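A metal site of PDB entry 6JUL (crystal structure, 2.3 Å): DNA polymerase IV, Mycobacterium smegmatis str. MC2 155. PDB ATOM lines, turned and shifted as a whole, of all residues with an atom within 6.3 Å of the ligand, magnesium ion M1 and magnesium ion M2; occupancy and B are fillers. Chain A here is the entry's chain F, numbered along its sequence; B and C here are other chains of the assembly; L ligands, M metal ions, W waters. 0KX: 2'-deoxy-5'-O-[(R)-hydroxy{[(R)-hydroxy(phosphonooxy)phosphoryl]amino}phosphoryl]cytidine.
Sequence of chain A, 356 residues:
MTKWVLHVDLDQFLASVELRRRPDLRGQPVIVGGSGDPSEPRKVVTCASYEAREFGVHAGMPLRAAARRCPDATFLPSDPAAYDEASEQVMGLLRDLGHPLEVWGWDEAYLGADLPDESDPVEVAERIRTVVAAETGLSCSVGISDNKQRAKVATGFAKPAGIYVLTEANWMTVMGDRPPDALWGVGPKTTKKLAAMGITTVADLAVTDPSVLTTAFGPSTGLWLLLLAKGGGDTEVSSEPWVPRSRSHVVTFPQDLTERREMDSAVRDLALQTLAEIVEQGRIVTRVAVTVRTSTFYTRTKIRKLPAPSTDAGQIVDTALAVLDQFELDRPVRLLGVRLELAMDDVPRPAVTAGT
Water W1 bridges O2B of the ligand and O of Thr 46.
Magnesium ion M1 is bound by OE2 of Glu 108 (2.2 Å), O3' of DC 18 of chain B (2.2 Å), OD2 of Asp 107 (2.2 Å), OD2 of Asp 9 (2.3 Å) and O2A of the ligand (2.3 Å).
Of the 24 residues printed, 4 come within 4 Å of magnesium ion M1.
NZ of Lys 159 touches magnesium ion M2, 3.98 Å away. Of the 24 residues printed, 4 come within 4 Å of magnesium ion M2. The nearest printed residue that does not touch magnesium ion M2 is Asp 11 (4.5 Å).
NZ of Lys 159 lies within hydrogen-bond range of O of Asp 9 (3.1 Å). NZ of Lys 152 lies within salt-bridge range of OE1 of Glu 108, at 2.9 Å. The side-chain carboxylate (OE1) of Glu 108 lies within hydrogen-bond range of a ring nitrogen (NE2) of His 7, at 2.9 Å. N of Tyr 50 lies within hydrogen-bond range of OE1 of Gln 12. NE of Arg 53 lies within hydrogen-bond range of O of Ala 48. The side-chain sulfur of Cys 47 sits close to the backbone carbonyl oxygen of Gln 12. The side-chain sulfur (SG) of Cys 47 is in hydrogen-bond range of the backbone NH (N) of Leu 14. The backbone NH (N) of Ala 15 sits at hydrogen-bond distance from the side-chain sulfur (SG) of Cys 47 (3.4 Å).
N4 of DC 18 of chain B is in hydrogen-bond range of a nitrogen (N4) of the ligand (3.3 Å). An oxygen (O3G) of the ligand sits at hydrogen-bond distance from the side-chain hydroxyl (OH) of Tyr 50, at 2.7 Å. NH1 of Arg 53 is in salt-bridge range of O2G of the ligand, at 2.8 Å. The backbone NH (N) of Gln 12 lies within hydrogen-bond range of an oxygen (O3G) of the ligand (2.8 Å). N4 of the ligand sits at hydrogen-bond distance from O6 of DG 4 of chain C (2.9 Å). O2 of the ligand sits at hydrogen-bond distance from OG1 of Thr 46. NZ of Lys 159 lies within salt-bridge range of O3G of the ligand (3.1 Å). The backbone NH (N) of Phe 13 lies within hydrogen-bond range of an oxygen (O2B) of the ligand (3.5 Å). The side-chain sulfur (SG) of Cys 47 is in hydrogen-bond range of an oxygen (O2B) of the ligand.
Merely in contact with the ligand: Asp 11, Leu 14, Ala 59 and DG 5 of chain C. Hydrophobic or aromatic side chains that line the ligand: Phe 13, Leu 14, Tyr 50 and Ala 59. 16 residues have an atom within 4 Å of the ligand: Asp 9, Leu 10, Asp 11, Gln 12, Phe 13, Leu 14, Thr 46, Cys 47, Tyr 50, Arg 53, Ala 59, Asp 107, Lys 159, DC 18 of chain B, DG 4 of chain C and DG 5 of chain C. The nearest printed residue that does not touch the ligand is Glu 108 (4.4 Å).
O2A of the ligand is bound to magnesium ion M2. OD1 of Asp 9 binds magnesium ion M2. Magnesium ion M2 is bound by an oxygen (O1B) of the ligand, 2.2 Å away. O1G of the ligand is bound to magnesium ion M2 (2.2 Å). Magnesium ion M2 is bound by O of Leu 10 (2.2 Å). OD1 of Asp 107 binds magnesium ion M2, at 2.3 Å. Magnesium ion M2 is bound by OD2 of Asp 107, at 2.3 Å. Magnesium ion M2 has seven donor atoms within binding distance.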
ATOM      1  N   HIS A   7      -0.405   6.600 -17.510  1.00  0.00           N
ATOM      2  CA  HIS A   7       0.157   5.275 -17.289  1.00  0.00           C
ATOM      3  C   HIS A   7      -0.430   4.614 -16.052  1.00  0.00           C
ATOM      4  O   HIS A   7      -0.249   5.118 -14.926  1.00  0.00           O
ATOM      5  CB  HIS A   7       1.708   5.312 -17.237  1.00  0.00           C
ATOM      6  CG  HIS A   7       2.320   3.978 -17.050  1.00  0.00           C
ATOM      7  ND1 HIS A   7       2.882   3.585 -15.861  1.00  0.00           N
ATOM      8  CD2 HIS A   7       2.301   2.887 -17.853  1.00  0.00           C
ATOM      9  CE1 HIS A   7       3.275   2.337 -15.964  1.00  0.00           C
ATOM     10  NE2 HIS A   7       2.965   1.885 -17.171  1.00  0.00           N
ATOM     11  N   ASP A   9      -0.461   1.491 -13.481  1.00  0.00           N
ATOM     12  CA  ASP A   9       0.347   0.410 -13.030  1.00  0.00           C
ATOM     13  C   ASP A   9      -0.200  -0.280 -11.715  1.00  0.00           C
ATOM     14  O   ASP A   9      -0.283   0.347 -10.719  1.00  0.00           O
ATOM     15  CB  ASP A   9       1.800   0.829 -12.947  1.00  0.00           C
ATOM     16  CG  ASP A   9       2.746  -0.325 -12.557  1.00  0.00           C
ATOM     17  OD1 ASP A   9       2.640  -0.800 -11.383  1.00  0.00           O
ATOM     18  OD2 ASP A   9       3.566  -0.776 -13.400  1.00  0.00           O
ATOM     19  N   LEU A  10      -0.568  -1.558 -11.772  1.00  0.00           N
ATOM     20  CA  LEU A  10      -0.999  -2.299 -10.571  1.00  0.00           C
ATOM     21  C   LEU A  10       0.058  -2.402  -9.445  1.00  0.00           C
ATOM     22  O   LEU A  10       1.295  -2.656  -9.714  1.00  0.00           O
ATOM     23  CB  LEU A  10      -1.468  -3.691 -11.006  1.00  0.00           C
ATOM     24  CG  LEU A  10      -2.804  -3.451 -11.731  1.00  0.00           C
ATOM     25  CD1 LEU A  10      -3.064  -4.624 -12.622  1.00  0.00           C
ATOM     26  CD2 LEU A  10      -3.924  -3.262 -10.669  1.00  0.00           C
ATOM     27  N   ASP A  11      -0.377  -2.087  -8.237  1.00  0.00           N
ATOM     28  CA  ASP A  11       0.474  -2.075  -7.037  1.00  0.00           C
ATOM     29  C   ASP A  11       0.802  -3.464  -6.611  1.00  0.00           C
ATOM     30  O   ASP A  11      -0.115  -4.288  -6.431  1.00  0.00           O
ATOM     31  CB  ASP A  11      -0.128  -1.293  -5.873  1.00  0.00           C
ATOM     32  CG  ASP A  11      -0.230   0.179  -6.147  1.00  0.00           C
ATOM     33  OD1 ASP A  11       0.374   0.743  -7.138  1.00  0.00           O
ATOM     34  OD2 ASP A  11      -0.948   0.827  -5.420  1.00  0.00           O
ATOM     35  N   GLN A  12       2.106  -3.747  -6.493  1.00  0.00           N
ATOM     36  CA  GLN A  12       2.652  -5.054  -6.007  1.00  0.00           C
ATOM     37  C   GLN A  12       1.791  -6.234  -6.573  1.00  0.00           C
ATOM     38  O   GLN A  12       1.239  -7.034  -5.834  1.00  0.00           O
ATOM     39  CB  GLN A  12       2.797  -5.047  -4.463  1.00  0.00           C
ATOM     40  CG  GLN A  12       1.441  -5.074  -3.697  1.00  0.00           C
ATOM     41  CD  GLN A  12       1.491  -5.144  -2.182  1.00  0.00           C
ATOM     42  OE1 GLN A  12       2.386  -5.720  -1.618  1.00  0.00           O
ATOM     43  NE2 GLN A  12       0.557  -4.527  -1.521  1.00  0.00           N
ATOM     44  N   PHE A  13       1.637  -6.232  -7.904  1.00  0.00           N
ATOM     45  CA  PHE A  13       0.602  -6.954  -8.583  1.00  0.00           C
ATOM     46  C   PHE A  13       0.450  -8.430  -8.092  1.00  0.00           C
ATOM     47  O   PHE A  13      -0.652  -8.801  -7.659  1.00  0.00           O
ATOM     48  CB  PHE A  13       0.822  -6.904 -10.058  1.00  0.00           C
ATOM     49  CG  PHE A  13      -0.194  -7.702 -10.844  1.00  0.00           C
ATOM     50  CD1 PHE A  13      -1.587  -7.547 -10.600  1.00  0.00           C
ATOM     51  CD2 PHE A  13       0.206  -8.618 -11.845  1.00  0.00           C
ATOM     52  CE1 PHE A  13      -2.514  -8.306 -11.312  1.00  0.00           C
ATOM     53  CE2 PHE A  13      -0.757  -9.387 -12.530  1.00  0.00           C
ATOM     54  CZ  PHE A  13      -2.110  -9.211 -12.281  1.00  0.00           C
ATOM     55  N   LEU A  14       1.484  -9.258  -8.123  1.00  0.00           N
ATOM     56  CA  LEU A  14       1.210 -10.697  -7.862  1.00  0.00           C
ATOM     57  C   LEU A  14       0.849 -10.872  -6.400  1.00  0.00           C
ATOM     58  O   LEU A  14      -0.099 -11.531  -6.057  1.00  0.00           O
ATOM     59  CB  LEU A  14       2.373 -11.574  -8.256  1.00  0.00           C
ATOM     60  CG  LEU A  14       2.696 -11.975  -9.721  1.00  0.00           C
ATOM     61  CD1 LEU A  14       2.505 -11.013 -10.812  1.00  0.00           C
ATOM     62  CD2 LEU A  14       4.157 -12.432  -9.773  1.00  0.00           C
ATOM     63  N   ALA A  15       1.582 -10.213  -5.532  1.00  0.00           N
ATOM     64  CA  ALA A  15       1.233 -10.232  -4.112  1.00  0.00           C
ATOM     65  C   ALA A  15      -0.215  -9.784  -3.844  1.00  0.00           C
ATOM     66  O   ALA A  15      -0.922 -10.401  -2.969  1.00  0.00           O
ATOM     67  CB  ALA A  15       2.201  -9.411  -3.298  1.00  0.00           C
ATOM     68  N   VAL A  45      12.710 -14.342  -6.417  1.00  0.00           N
ATOM     69  CA  VAL A  45      11.526 -13.585  -6.139  1.00  0.00           C
ATOM     70  C   VAL A  45      11.014 -12.914  -7.398  1.00  0.00           C
ATOM     71  O   VAL A  45      11.745 -12.248  -8.170  1.00  0.00           O
ATOM     72  CB  VAL A  45      11.746 -12.524  -5.064  1.00  0.00           C
ATOM     73  CG1 VAL A  45      10.477 -11.648  -4.896  1.00  0.00           C
ATOM     74  CG2 VAL A  45      12.182 -13.140  -3.710  1.00  0.00           C
ATOM     75  N   THR A  46       9.720 -13.091  -7.583  1.00  0.00           N
ATOM     76  CA  THR A  46       9.071 -12.436  -8.672  1.00  0.00           C
ATOM     77  C   THR A  46       8.176 -11.211  -8.282  1.00  0.00           C
ATOM     78  O   THR A  46       8.094 -10.271  -9.017  1.00  0.00           O
ATOM     79  CB  THR A  46       8.432 -13.509  -9.511  1.00  0.00           C
ATOM     80  OG1 THR A  46       8.383 -12.960 -10.776  1.00  0.00           O
ATOM     81  CG2 THR A  46       7.065 -13.809  -9.057  1.00  0.00           C
ATOM     82  N   CYS A  47       7.589 -11.206  -7.079  1.00  0.00           N
ATOM     83  CA  CYS A  47       6.899 -10.122  -6.539  1.00  0.00           C
ATOM     84  C   CYS A  47       6.914 -10.229  -5.032  1.00  0.00           C
ATOM     85  O   CYS A  47       6.324 -11.153  -4.443  1.00  0.00           O
ATOM     86  CB  CYS A  47       5.448 -10.080  -7.048  1.00  0.00           C
ATOM     87  SG  CYS A  47       4.546  -8.719  -6.206  1.00  0.00           S
ATOM     88  N   ALA A  48       7.548  -9.281  -4.402  1.00  0.00           N
ATOM     89  CA  ALA A  48       7.540  -9.220  -2.936  1.00  0.00           C
ATOM     90  C   ALA A  48       6.436  -8.242  -2.584  1.00  0.00           C
ATOM     91  O   ALA A  48       6.271  -7.194  -3.290  1.00  0.00           O
ATOM     92  CB  ALA A  48       8.877  -8.706  -2.465  1.00  0.00           C
ATOM     93  N   TYR A  50       4.774  -5.212  -0.433  1.00  0.00           N
ATOM     94  CA  TYR A  50       5.409  -4.064   0.235  1.00  0.00           C
ATOM     95  C   TYR A  50       6.063  -4.379   1.564  1.00  0.00           C
ATOM     96  O   TYR A  50       7.128  -3.785   1.865  1.00  0.00           O
ATOM     97  CB  TYR A  50       4.506  -2.857   0.331  1.00  0.00           C
ATOM     98  CG  TYR A  50       4.039  -2.321  -1.023  1.00  0.00           C
ATOM     99  CD1 TYR A  50       4.793  -2.510  -2.167  1.00  0.00           C
ATOM    100  CD2 TYR A  50       2.869  -1.594  -1.124  1.00  0.00           C
ATOM    101  CE1 TYR A  50       4.426  -2.001  -3.421  1.00  0.00           C
ATOM    102  CE2 TYR A  50       2.445  -1.014  -2.363  1.00  0.00           C
ATOM    103  CZ  TYR A  50       3.222  -1.235  -3.530  1.00  0.00           C
ATOM    104  OH  TYR A  50       2.856  -0.673  -4.759  1.00  0.00           O
ATOM    105  N   ARG A  53       9.340  -5.818   1.088  1.00  0.00           N
ATOM    106  CA  ARG A  53      10.368  -4.899   0.456  1.00  0.00           C
ATOM    107  C   ARG A  53      11.000  -4.118   1.603  1.00  0.00           C
ATOM    108  O   ARG A  53      12.128  -3.668   1.510  1.00  0.00           O
ATOM    109  CB  ARG A  53       9.751  -3.943  -0.621  1.00  0.00           C
ATOM    110  CG  ARG A  53       9.301  -4.679  -1.929  1.00  0.00           C
ATOM    111  CD  ARG A  53       8.586  -3.831  -2.976  1.00  0.00           C
ATOM    112  NE  ARG A  53       7.592  -4.592  -3.801  1.00  0.00           N
ATOM    113  CZ  ARG A  53       7.091  -4.225  -5.002  1.00  0.00           C
ATOM    114  NH1 ARG A  53       7.341  -3.056  -5.526  1.00  0.00           N
ATOM    115  NH2 ARG A  53       6.195  -4.999  -5.621  1.00  0.00           N
ATOM    116  N   ALA A  59      12.046  -8.000  -6.693  1.00  0.00           N
ATOM    117  CA  ALA A  59      12.000  -8.849  -7.887  1.00  0.00           C
ATOM    118  C   ALA A  59      13.412  -9.133  -8.341  1.00  0.00           C
ATOM    119  O   ALA A  59      14.129  -8.193  -8.571  1.00  0.00           O
ATOM    120  CB  ALA A  59      11.193  -8.152  -9.006  1.00  0.00           C
ATOM    121  N   GLY A  60      13.792 -10.422  -8.520  1.00  0.00           N
ATOM    122  CA  GLY A  60      15.064 -10.833  -9.164  1.00  0.00           C
ATOM    123  C   GLY A  60      15.989 -11.359  -8.081  1.00  0.00           C
ATOM    124  O   GLY A  60      16.976 -12.085  -8.350  1.00  0.00           O
ATOM    125  N   TRP A 106       1.125  -8.049 -17.984  1.00  0.00           N
ATOM    126  CA  TRP A 106       0.062  -8.322 -17.044  1.00  0.00           C
ATOM    127  C   TRP A 106      -0.423  -7.013 -16.428  1.00  0.00           C
ATOM    128  O   TRP A 106      -1.606  -6.899 -16.223  1.00  0.00           O
ATOM    129  CB  TRP A 106       0.574  -9.182 -15.894  1.00  0.00           C
ATOM    130  CG  TRP A 106       0.569 -10.662 -16.039  1.00  0.00           C
ATOM    131  CD1 TRP A 106      -0.369 -11.479 -16.705  1.00  0.00           C
ATOM    132  CD2 TRP A 106       1.454 -11.566 -15.382  1.00  0.00           C
ATOM    133  NE1 TRP A 106      -0.061 -12.813 -16.541  1.00  0.00           N
ATOM    134  CE2 TRP A 106       1.066 -12.897 -15.749  1.00  0.00           C
ATOM    135  CE3 TRP A 106       2.611 -11.377 -14.600  1.00  0.00           C
ATOM    136  CZ2 TRP A 106       1.730 -14.007 -15.295  1.00  0.00           C
ATOM    137  CZ3 TRP A 106       3.299 -12.470 -14.173  1.00  0.00           C
ATOM    138  CH2 TRP A 106       2.863 -13.778 -14.511  1.00  0.00           C
ATOM    139  N   ASP A 107       0.493  -6.061 -16.179  1.00  0.00           N
ATOM    140  CA  ASP A 107       0.431  -5.171 -15.004  1.00  0.00           C
ATOM    141  C   ASP A 107       0.142  -3.758 -15.393  1.00  0.00           C
ATOM    142  O   ASP A 107      -0.212  -2.919 -14.514  1.00  0.00           O
ATOM    143  CB  ASP A 107       1.879  -5.133 -14.356  1.00  0.00           C
ATOM    144  CG  ASP A 107       2.018  -4.110 -13.196  1.00  0.00           C
ATOM    145  OD1 ASP A 107       1.552  -4.293 -12.087  1.00  0.00           O
ATOM    146  OD2 ASP A 107       2.609  -3.012 -13.310  1.00  0.00           O
ATOM    147  N   GLU A 108       0.425  -3.443 -16.671  1.00  0.00           N
ATOM    148  CA  GLU A 108       0.402  -2.057 -17.104  1.00  0.00           C
ATOM    149  C   GLU A 108      -0.235  -1.700 -18.480  1.00  0.00           C
ATOM    150  O   GLU A 108      -0.409  -2.533 -19.362  1.00  0.00           O
ATOM    151  CB  GLU A 108       1.797  -1.445 -17.066  1.00  0.00           C
ATOM    152  CG  GLU A 108       2.940  -2.355 -17.256  1.00  0.00           C
ATOM    153  CD  GLU A 108       4.154  -1.509 -17.138  1.00  0.00           C
ATOM    154  OE1 GLU A 108       4.246  -0.546 -17.953  1.00  0.00           O
ATOM    155  OE2 GLU A 108       4.958  -1.710 -16.173  1.00  0.00           O
ATOM    156  N   LYS A 152       5.550   7.177 -17.290  1.00  0.00           N
ATOM    157  CA  LYS A 152       6.098   6.011 -16.704  1.00  0.00           C
ATOM    158  C   LYS A 152       6.914   6.507 -15.527  1.00  0.00           C
ATOM    159  O   LYS A 152       6.710   6.044 -14.412  1.00  0.00           O
ATOM    160  CB  LYS A 152       6.856   5.235 -17.828  1.00  0.00           C
ATOM    161  CG  LYS A 152       7.452   3.948 -17.423  1.00  0.00           C
ATOM    162  CD  LYS A 152       6.341   2.932 -17.288  1.00  0.00           C
ATOM    163  CE  LYS A 152       6.777   1.495 -17.658  1.00  0.00           C
ATOM    164  NZ  LYS A 152       6.460   0.562 -16.523  1.00  0.00           N
ATOM    165  N   LYS A 159       3.588   6.028  -6.838  1.00  0.00           N
ATOM    166  CA  LYS A 159       3.646   4.820  -5.973  1.00  0.00           C
ATOM    167  C   LYS A 159       3.758   5.201  -4.464  1.00  0.00           C
ATOM    168  O   LYS A 159       4.582   6.078  -4.111  1.00  0.00           O
ATOM    169  CB  LYS A 159       4.862   3.902  -6.317  1.00  0.00           C
ATOM    170  CG  LYS A 159       4.723   3.065  -7.613  1.00  0.00           C
ATOM    171  CD  LYS A 159       3.644   2.002  -7.515  1.00  0.00           C
ATOM    172  CE  LYS A 159       3.378   1.481  -8.932  1.00  0.00           C
ATOM    173  NZ  LYS A 159       2.298   0.411  -9.028  1.00  0.00           N
ATOM    174  P    DC B  18       9.621  -1.251 -16.098  1.00  0.00           P
ATOM    175  OP1  DC B  18       8.742  -0.093 -16.050  1.00  0.00           O
ATOM    176  OP2  DC B  18      10.645  -1.487 -15.064  1.00  0.00           O
ATOM    177  O5'  DC B  18       8.813  -2.615 -16.204  1.00  0.00           O
ATOM    178  C5'  DC B  18       7.836  -2.852 -17.269  1.00  0.00           C
ATOM    179  C4'  DC B  18       7.251  -4.238 -17.096  1.00  0.00           C
ATOM    180  O4'  DC B  18       8.271  -5.198 -17.443  1.00  0.00           O
ATOM    181  C3'  DC B  18       6.866  -4.534 -15.639  1.00  0.00           C
ATOM    182  O3'  DC B  18       5.475  -4.295 -15.351  1.00  0.00           O
ATOM    183  C2'  DC B  18       7.231  -5.984 -15.468  1.00  0.00           C
ATOM    184  C1'  DC B  18       8.185  -6.321 -16.612  1.00  0.00           C
ATOM    185  N1   DC B  18       9.554  -6.731 -16.257  1.00  0.00           N
ATOM    186  C2   DC B  18       9.878  -8.065 -16.451  1.00  0.00           C
ATOM    187  O2   DC B  18       9.005  -8.824 -16.869  1.00  0.00           O
ATOM    188  N3   DC B  18      11.154  -8.484 -16.253  1.00  0.00           N
ATOM    189  C4   DC B  18      12.070  -7.620 -15.784  1.00  0.00           C
ATOM    190  N4   DC B  18      13.311  -8.081 -15.543  1.00  0.00           N
ATOM    191  C5   DC B  18      11.759  -6.249 -15.543  1.00  0.00           C
ATOM    192  C6   DC B  18      10.493  -5.847 -15.786  1.00  0.00           C
ATOM    193  P    DG C   4      19.353 -16.649 -12.728  1.00  0.00           P
ATOM    194  OP1  DG C   4      20.006 -17.948 -12.902  1.00  0.00           O
ATOM    195  OP2  DG C   4      19.473 -15.603 -13.727  1.00  0.00           O
ATOM    196  O5'  DG C   4      17.784 -16.833 -12.538  1.00  0.00           O
ATOM    197  C5'  DG C   4      17.194 -17.862 -11.754  1.00  0.00           C
ATOM    198  C4'  DG C   4      15.851 -18.198 -12.364  1.00  0.00           C
ATOM    199  O4'  DG C   4      14.969 -17.063 -12.210  1.00  0.00           O
ATOM    200  C3'  DG C   4      15.897 -18.490 -13.855  1.00  0.00           C
ATOM    201  O3'  DG C   4      14.982 -19.560 -14.163  1.00  0.00           O
ATOM    202  C2'  DG C   4      15.552 -17.133 -14.483  1.00  0.00           C
ATOM    203  C1'  DG C   4      14.612 -16.515 -13.453  1.00  0.00           C
ATOM    204  N9   DG C   4      14.705 -15.079 -13.280  1.00  0.00           N
ATOM    205  C8   DG C   4      15.853 -14.400 -12.950  1.00  0.00           C
ATOM    206  N7   DG C   4      15.675 -13.126 -12.797  1.00  0.00           N
ATOM    207  C5   DG C   4      14.313 -12.949 -13.001  1.00  0.00           C
ATOM    208  C6   DG C   4      13.534 -11.769 -12.924  1.00  0.00           C
ATOM    209  O6   DG C   4      13.897 -10.615 -12.684  1.00  0.00           O
ATOM    210  N1   DG C   4      12.204 -12.024 -13.214  1.00  0.00           N
ATOM    211  C2   DG C   4      11.669 -13.256 -13.510  1.00  0.00           C
ATOM    212  N2   DG C   4      10.335 -13.272 -13.720  1.00  0.00           N
ATOM    213  N3   DG C   4      12.383 -14.380 -13.511  1.00  0.00           N
ATOM    214  C4   DG C   4      13.694 -14.147 -13.267  1.00  0.00           C
ATOM    215  P    DG C   5      14.815 -20.034 -15.694  1.00  0.00           P
ATOM    216  OP1  DG C   5      14.486 -21.448 -15.722  1.00  0.00           O
ATOM    217  OP2  DG C   5      16.040 -19.620 -16.488  1.00  0.00           O
ATOM    218  O5'  DG C   5      13.605 -19.090 -16.157  1.00  0.00           O
ATOM    219  C5'  DG C   5      12.255 -19.208 -15.717  1.00  0.00           C
ATOM    220  C4'  DG C   5      11.422 -18.319 -16.616  1.00  0.00           C
ATOM    221  O4'  DG C   5      11.686 -16.946 -16.271  1.00  0.00           O
ATOM    222  C3'  DG C   5      11.669 -18.454 -18.117  1.00  0.00           C
ATOM    223  O3'  DG C   5      10.391 -18.543 -18.734  1.00  0.00           O
ATOM    224  C2'  DG C   5      12.416 -17.180 -18.501  1.00  0.00           C
ATOM    225  C1'  DG C   5      11.848 -16.205 -17.486  1.00  0.00           C
ATOM    226  N9   DG C   5      12.657 -15.019 -17.198  1.00  0.00           N
ATOM    227  C8   DG C   5      14.008 -14.981 -17.009  1.00  0.00           C
ATOM    228  N7   DG C   5      14.457 -13.778 -16.754  1.00  0.00           N
ATOM    229  C5   DG C   5      13.317 -12.980 -16.754  1.00  0.00           C
ATOM    230  C6   DG C   5      13.161 -11.571 -16.490  1.00  0.00           C
ATOM    231  O6   DG C   5      14.029 -10.736 -16.244  1.00  0.00           O
ATOM    232  N1   DG C   5      11.831 -11.188 -16.589  1.00  0.00           N
ATOM    233  C2   DG C   5      10.778 -12.020 -16.880  1.00  0.00           C
ATOM    234  N2   DG C   5       9.565 -11.459 -16.888  1.00  0.00           N
ATOM    235  N3   DG C   5      10.901 -13.326 -17.051  1.00  0.00           N
ATOM    236  C4   DG C   5      12.199 -13.736 -16.994  1.00  0.00           C
HETATM  237  PG  0KX L   1       4.902  -2.143  -8.061  1.00  0.00           P
HETATM  238  O1G 0KX L   1       4.320  -2.004  -9.530  1.00  0.00           O
HETATM  239  O2G 0KX L   1       6.253  -1.643  -7.648  1.00  0.00           O
HETATM  240  O3G 0KX L   1       3.796  -1.613  -7.140  1.00  0.00           O
HETATM  241  PB  0KX L   1       4.945  -4.870  -9.051  1.00  0.00           P
HETATM  242  O1B 0KX L   1       3.612  -4.603  -9.786  1.00  0.00           O
HETATM  243  O2B 0KX L   1       5.045  -6.280  -8.515  1.00  0.00           O
HETATM  244  O3B 0KX L   1       5.000  -3.760  -7.904  1.00  0.00           O
HETATM  245  PA  0KX L   1       6.165  -4.171 -11.701  1.00  0.00           P
HETATM  246  O1A 0KX L   1       7.503  -3.566 -11.892  1.00  0.00           O
HETATM  247  O2A 0KX L   1       4.871  -3.415 -12.078  1.00  0.00           O
HETATM  248  N3A 0KX L   1       6.157  -4.448 -10.061  1.00  0.00           N
HETATM  249  O5' 0KX L   1       6.145  -5.601 -12.395  1.00  0.00           O
HETATM  250  C5' 0KX L   1       4.835  -6.241 -12.447  1.00  0.00           C
HETATM  251  C4' 0KX L   1       4.845  -7.749 -12.432  1.00  0.00           C
HETATM  252  O4' 0KX L   1       5.788  -8.148 -13.413  1.00  0.00           O
HETATM  253  C3' 0KX L   1       5.339  -8.278 -11.114  1.00  0.00           C
HETATM  254  O3' 0KX L   1       4.405  -8.287 -10.028  1.00  0.00           O
HETATM  255  C2' 0KX L   1       5.907  -9.615 -11.486  1.00  0.00           C
HETATM  256  C1' 0KX L   1       6.440  -9.317 -12.913  1.00  0.00           C
HETATM  257  N1  0KX L   1       7.895  -9.015 -12.821  1.00  0.00           N
HETATM  258  C2  0KX L   1       8.819 -10.038 -12.945  1.00  0.00           C
HETATM  259  N3  0KX L   1      10.121  -9.747 -12.885  1.00  0.00           N
HETATM  260  C4  0KX L   1      10.638  -8.516 -12.660  1.00  0.00           C
HETATM  261  C5  0KX L   1       9.783  -7.419 -12.520  1.00  0.00           C
HETATM  262  C6  0KX L   1       8.403  -7.733 -12.581  1.00  0.00           C
HETATM  263  O2  0KX L   1       8.462 -11.204 -13.089  1.00  0.00           O
HETATM  264  N4  0KX L   1      11.981  -8.397 -12.584  1.00  0.00           N
HETATM  265 MG    MG M   1       4.618  -2.613 -14.181  1.00  0.00          MG
HETATM  266 MG    MG M   2       3.037  -2.926 -11.068  1.00  0.00          MG
HETATM  267  O   HOH W   1       7.830  -7.333  -8.457  1.00  0.00           O
HETATM  268  O   HOH W   2       5.847  -0.427 -11.258  1.00  0.00           O
